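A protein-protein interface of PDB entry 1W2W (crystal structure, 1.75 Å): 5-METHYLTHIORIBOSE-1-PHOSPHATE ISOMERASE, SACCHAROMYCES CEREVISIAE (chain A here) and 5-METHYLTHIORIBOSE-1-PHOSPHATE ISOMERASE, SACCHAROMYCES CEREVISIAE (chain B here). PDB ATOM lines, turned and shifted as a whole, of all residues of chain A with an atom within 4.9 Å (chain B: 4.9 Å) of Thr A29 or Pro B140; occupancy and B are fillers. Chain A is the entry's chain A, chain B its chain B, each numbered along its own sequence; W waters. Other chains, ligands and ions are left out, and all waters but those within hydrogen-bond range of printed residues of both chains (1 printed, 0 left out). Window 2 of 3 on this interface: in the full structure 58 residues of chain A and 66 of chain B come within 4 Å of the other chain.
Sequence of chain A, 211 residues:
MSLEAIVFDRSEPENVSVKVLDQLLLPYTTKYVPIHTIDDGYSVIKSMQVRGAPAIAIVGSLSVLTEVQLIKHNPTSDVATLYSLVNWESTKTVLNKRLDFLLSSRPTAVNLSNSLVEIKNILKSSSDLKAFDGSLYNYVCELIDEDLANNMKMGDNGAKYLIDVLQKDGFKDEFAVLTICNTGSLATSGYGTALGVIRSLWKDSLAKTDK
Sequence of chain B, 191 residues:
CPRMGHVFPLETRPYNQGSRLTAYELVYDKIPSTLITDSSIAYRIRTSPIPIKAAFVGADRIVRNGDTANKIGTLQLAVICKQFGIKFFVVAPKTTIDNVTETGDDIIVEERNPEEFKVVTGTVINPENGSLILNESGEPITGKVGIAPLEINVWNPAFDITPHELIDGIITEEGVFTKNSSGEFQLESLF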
ATOM      1  N   ASP A  22      28.079   4.213  -7.117  1.00  0.00           N
ATOM      2  CA  ASP A  22      26.627   4.162  -6.975  1.00  0.00           C
ATOM      3  C   ASP A  22      26.125   2.804  -7.468  1.00  0.00           C
ATOM      4  O   ASP A  22      25.983   2.563  -8.683  1.00  0.00           O
ATOM      5  CB  ASP A  22      25.979   5.283  -7.780  1.00  0.00           C
ATOM      6  CG  ASP A  22      24.502   5.411  -7.496  1.00  0.00           C
ATOM      7  OD1 ASP A  22      23.898   4.412  -7.031  1.00  0.00           O
ATOM      8  OD2 ASP A  22      23.873   6.477  -7.691  1.00  0.00           O
ATOM      9  N   LEU A  25      23.305   2.001 -10.055  1.00  0.00           N
ATOM     10  CA  LEU A  25      23.505   2.280 -11.477  1.00  0.00           C
ATOM     11  C   LEU A  25      24.358   1.238 -12.212  1.00  0.00           C
ATOM     12  O   LEU A  25      24.448   1.254 -13.448  1.00  0.00           O
ATOM     13  CB  LEU A  25      24.103   3.681 -11.649  1.00  0.00           C
ATOM     14  CG  LEU A  25      23.319   4.802 -10.952  1.00  0.00           C
ATOM     15  CD1 LEU A  25      23.973   6.154 -11.229  1.00  0.00           C
ATOM     16  CD2 LEU A  25      21.857   4.808 -11.392  1.00  0.00           C
ATOM     17  N   LEU A  26      24.977   0.326 -11.456  1.00  0.00           N
ATOM     18  CA  LEU A  26      25.787  -0.732 -12.050  1.00  0.00           C
ATOM     19  C   LEU A  26      24.876  -1.745 -12.753  1.00  0.00           C
ATOM     20  O   LEU A  26      23.689  -1.824 -12.434  1.00  0.00           O
ATOM     21  CB  LEU A  26      26.624  -1.430 -10.970  1.00  0.00           C
ATOM     22  CG  LEU A  26      27.739  -0.617 -10.284  1.00  0.00           C
ATOM     23  CD1 LEU A  26      28.259  -1.344  -9.031  1.00  0.00           C
ATOM     24  CD2 LEU A  26      28.889  -0.391 -11.242  1.00  0.00           C
ATOM     25  N   PRO A  27      25.398  -2.530 -13.691  1.00  0.00           N
ATOM     26  CA  PRO A  27      26.804  -2.522 -14.098  1.00  0.00           C
ATOM     27  C   PRO A  27      27.159  -1.608 -15.263  1.00  0.00           C
ATOM     28  O   PRO A  27      28.352  -1.434 -15.530  1.00  0.00           O
ATOM     29  CB  PRO A  27      27.025  -3.975 -14.522  1.00  0.00           C
ATOM     30  CG  PRO A  27      25.712  -4.368 -15.120  1.00  0.00           C
ATOM     31  CD  PRO A  27      24.627  -3.558 -14.413  1.00  0.00           C
ATOM     32  N   TYR A  28      26.179  -1.044 -15.959  1.00  0.00           N
ATOM     33  CA  TYR A  28      26.526  -0.293 -17.166  1.00  0.00           C
ATOM     34  C   TYR A  28      27.031   1.108 -16.897  1.00  0.00           C
ATOM     35  O   TYR A  28      27.770   1.668 -17.707  1.00  0.00           O
ATOM     36  CB  TYR A  28      25.358  -0.235 -18.142  1.00  0.00           C
ATOM     37  CG  TYR A  28      25.072  -1.575 -18.789  1.00  0.00           C
ATOM     38  CD1 TYR A  28      25.781  -2.004 -19.913  1.00  0.00           C
ATOM     39  CD2 TYR A  28      24.091  -2.416 -18.264  1.00  0.00           C
ATOM     40  CE1 TYR A  28      25.513  -3.234 -20.494  1.00  0.00           C
ATOM     41  CE2 TYR A  28      23.819  -3.641 -18.843  1.00  0.00           C
ATOM     42  CZ  TYR A  28      24.525  -4.044 -19.950  1.00  0.00           C
ATOM     43  OH  TYR A  28      24.222  -5.273 -20.500  1.00  0.00           O
ATOM     44  N   THR A  29      26.621   1.672 -15.768  1.00  0.00           N
ATOM     45  CA  THR A  29      27.025   3.028 -15.412  1.00  0.00           C
ATOM     46  C   THR A  29      27.940   2.980 -14.208  1.00  0.00           C
ATOM     47  O   THR A  29      27.609   2.358 -13.195  1.00  0.00           O
ATOM     48  CB  THR A  29      25.781   3.863 -15.104  1.00  0.00           C
ATOM     49  OG1 THR A  29      25.065   4.066 -16.318  1.00  0.00           O
ATOM     50  CG2 THR A  29      26.145   5.287 -14.674  1.00  0.00           C
ATOM     51  N   THR A  30      29.095   3.627 -14.335  1.00  0.00           N
ATOM     52  CA  THR A  30      30.054   3.694 -13.246  1.00  0.00           C
ATOM     53  C   THR A  30      30.074   5.141 -12.809  1.00  0.00           C
ATOM     54  O   THR A  30      30.644   5.988 -13.496  1.00  0.00           O
ATOM     55  CB  THR A  30      31.446   3.245 -13.747  1.00  0.00           C
ATOM     56  OG1 THR A  30      31.458   1.814 -13.833  1.00  0.00           O
ATOM     57  CG2 THR A  30      32.524   3.530 -12.705  1.00  0.00           C
ATOM     58  N   LYS A  31      29.437   5.430 -11.680  1.00  0.00           N
ATOM     59  CA  LYS A  31      29.341   6.800 -11.199  1.00  0.00           C
ATOM     60  C   LYS A  31      29.737   6.856  -9.727  1.00  0.00           C
ATOM     61  O   LYS A  31      29.269   6.038  -8.937  1.00  0.00           O
ATOM     62  CB  LYS A  31      27.906   7.307 -11.349  1.00  0.00           C
ATOM     63  CG  LYS A  31      27.613   8.575 -10.582  1.00  0.00           C
ATOM     64  CD  LYS A  31      26.595   9.428 -11.310  1.00  0.00           C
ATOM     65  CE  LYS A  31      26.191  10.654 -10.486  1.00  0.00           C
ATOM     66  NZ  LYS A  31      27.349  11.572 -10.226  1.00  0.00           N
ATOM     67  N   THR B 123      19.626  -0.184 -17.300  1.00  0.00           N
ATOM     68  CA  THR B 123      20.142   0.690 -18.350  1.00  0.00           C
ATOM     69  C   THR B 123      19.109   0.759 -19.490  1.00  0.00           C
ATOM     70  O   THR B 123      18.557  -0.265 -19.885  1.00  0.00           O
ATOM     71  CB  THR B 123      21.545   0.185 -18.780  1.00  0.00           C
ATOM     72  OG1 THR B 123      22.305   1.254 -19.368  1.00  0.00           O
ATOM     73  CG2 THR B 123      21.482  -0.912 -19.857  1.00  0.00           C
ATOM     74  N   LEU B 132      22.341  -0.247 -26.194  1.00  0.00           N
ATOM     75  CA  LEU B 132      22.296   0.715 -25.107  1.00  0.00           C
ATOM     76  C   LEU B 132      21.972   2.107 -25.642  1.00  0.00           C
ATOM     77  O   LEU B 132      22.520   2.529 -26.674  1.00  0.00           O
ATOM     78  CB  LEU B 132      23.639   0.733 -24.369  1.00  0.00           C
ATOM     79  CG  LEU B 132      24.227  -0.634 -24.000  1.00  0.00           C
ATOM     80  CD1 LEU B 132      25.641  -0.501 -23.408  1.00  0.00           C
ATOM     81  CD2 LEU B 132      23.293  -1.351 -23.024  1.00  0.00           C
ATOM     82  N   ILE B 133      21.077   2.807 -24.947  1.00  0.00           N
ATOM     83  CA  ILE B 133      20.903   4.236 -25.154  1.00  0.00           C
ATOM     84  C   ILE B 133      21.933   5.001 -24.329  1.00  0.00           C
ATOM     85  O   ILE B 133      21.997   4.836 -23.111  1.00  0.00           O
ATOM     86  CB  ILE B 133      19.473   4.665 -24.787  1.00  0.00           C
ATOM     87  CG1 ILE B 133      18.479   4.098 -25.809  1.00  0.00           C
ATOM     88  CG2 ILE B 133      19.355   6.179 -24.708  1.00  0.00           C
ATOM     89  CD1 ILE B 133      18.557   4.760 -27.170  1.00  0.00           C
ATOM     90  N   LEU B 134      22.738   5.827 -25.002  1.00  0.00           N
ATOM     91  CA  LEU B 134      23.820   6.562 -24.344  1.00  0.00           C
ATOM     92  C   LEU B 134      23.534   8.052 -24.369  1.00  0.00           C
ATOM     93  O   LEU B 134      22.863   8.551 -25.282  1.00  0.00           O
ATOM     94  CB  LEU B 134      25.172   6.287 -25.025  1.00  0.00           C
ATOM     95  CG  LEU B 134      25.575   4.861 -25.394  1.00  0.00           C
ATOM     96  CD1 LEU B 134      26.868   4.808 -26.184  1.00  0.00           C
ATOM     97  CD2 LEU B 134      25.699   3.954 -24.170  1.00  0.00           C
ATOM     98  N   GLY B 138      28.508   9.615 -23.979  1.00  0.00           N
ATOM     99  CA  GLY B 138      28.788   8.232 -24.314  1.00  0.00           C
ATOM    100  C   GLY B 138      28.479   7.268 -23.179  1.00  0.00           C
ATOM    101  O   GLY B 138      28.819   6.091 -23.240  1.00  0.00           O
ATOM    102  N   GLU B 139      27.836   7.760 -22.130  1.00  0.00           N
ATOM    103  CA  GLU B 139      27.573   6.879 -21.005  1.00  0.00           C
ATOM    104  C   GLU B 139      26.133   6.377 -21.018  1.00  0.00           C
ATOM    105  O   GLU B 139      25.199   7.118 -21.333  1.00  0.00           O
ATOM    106  CB  GLU B 139      27.958   7.523 -19.673  1.00  0.00           C
ATOM    107  CG  GLU B 139      26.990   8.585 -19.191  1.00  0.00           C
ATOM    108  CD  GLU B 139      27.499   9.338 -17.970  1.00  0.00           C
ATOM    109  OE1 GLU B 139      27.135   8.936 -16.832  1.00  0.00           O
ATOM    110  OE2 GLU B 139      28.252  10.327 -18.160  1.00  0.00           O
ATOM    111  N   PRO B 140      25.977   5.100 -20.688  1.00  0.00           N
ATOM    112  CA  PRO B 140      24.652   4.471 -20.593  1.00  0.00           C
ATOM    113  C   PRO B 140      23.701   5.259 -19.706  1.00  0.00           C
ATOM    114  O   PRO B 140      24.094   5.720 -18.636  1.00  0.00           O
ATOM    115  CB  PRO B 140      24.975   3.111 -19.982  1.00  0.00           C
ATOM    116  CG  PRO B 140      26.352   2.828 -20.501  1.00  0.00           C
ATOM    117  CD  PRO B 140      27.066   4.156 -20.399  1.00  0.00           C
ATOM    118  N   ILE B 141      22.457   5.421 -20.149  1.00  0.00           N
ATOM    119  CA  ILE B 141      21.471   6.190 -19.396  1.00  0.00           C
ATOM    120  C   ILE B 141      20.684   5.220 -18.513  1.00  0.00           C
ATOM    121  O   ILE B 141      20.280   4.138 -18.957  1.00  0.00           O
ATOM    122  CB  ILE B 141      20.547   6.971 -20.364  1.00  0.00           C
ATOM    123  CG1 ILE B 141      21.315   8.135 -21.006  1.00  0.00           C
ATOM    124  CG2 ILE B 141      19.328   7.542 -19.647  1.00  0.00           C
ATOM    125  CD1 ILE B 141      20.634   8.718 -22.231  1.00  0.00           C
ATOM    126  N   THR B 142      20.493   5.605 -17.257  1.00  0.00           N
ATOM    127  CA  THR B 142      19.666   4.822 -16.340  1.00  0.00           C
ATOM    128  C   THR B 142      18.186   5.089 -16.625  1.00  0.00           C
ATOM    129  O   THR B 142      17.769   6.210 -16.944  1.00  0.00           O
ATOM    130  CB  THR B 142      20.052   5.156 -14.876  1.00  0.00           C
ATOM    131  OG1 THR B 142      19.280   4.351 -13.962  1.00  0.00           O
ATOM    132  CG2 THR B 142      19.659   6.580 -14.535  1.00  0.00           C
HETATM  133  O   HOH W   1      22.918   2.187 -16.773  1.00  0.00           O
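Of the 8 printed residues of chain A, 3 touch a printed residue of chain B.
Hydrophobic or aromatic side chains of chain A within 4 Å of the printed part of chain B: Leu A25 and Tyr A28.
Printed residues of chain B that touch a printed residue of chain A: Thr B123, Leu B132, Pro B140 and Thr B142.
Hydrophobic or aromatic side chains of chain B that line the printed part of chain A: Leu B132 and Pro B140.
Among the printed residues, no Asp or Glu carboxylate lies within 4 Å of a Lys or Arg side-chain nitrogen of the other chain.
Among the printed residues, pairs that only touch across the chains: Leu A25 with Thr B142 (3.7 Å), Tyr A28 with Thr B123 (3.4 Å), Tyr A28 with Leu B132 (3.8 Å) and Tyr A28 with Pro B140 (3.3 Å).
The side-chain hydroxyl (OG1) of Thr A29 is in hydrogen-bond range of the backbone carbonyl oxygen (O) of Pro B140.
Water W1 bridges the side-chain hydroxyl (OG1) of Thr B123 (2.8 Å) and the side-chain hydroxyl (OG1) of Thr A29 (2.9 Å).
Of chain B, only Pro B140 (3.0 Å) comes within 4 Å of Thr A29.
Pro B140 touches just these residues of chain A: Tyr A28 (3.3 Å) and Thr A29 (3.0 Å).
Of the printed residues of chain B, Tyr A28 touches Thr B123 (3.4 Å), Leu B132 (3.8 Å) and Pro B140 (3.3 Å).
Of the printed residues of chain B, Leu A25 touches Thr B142.
Printed residues of chain A within 4 Å of Thr B123: Tyr A28 (3.4 Å).
Printed residues of chain A within 4 Å of Leu B132: Tyr A28 (3.8 Å).
Of the printed residues of chain A, Thr B142 touches Leu A25 (3.7 Å).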
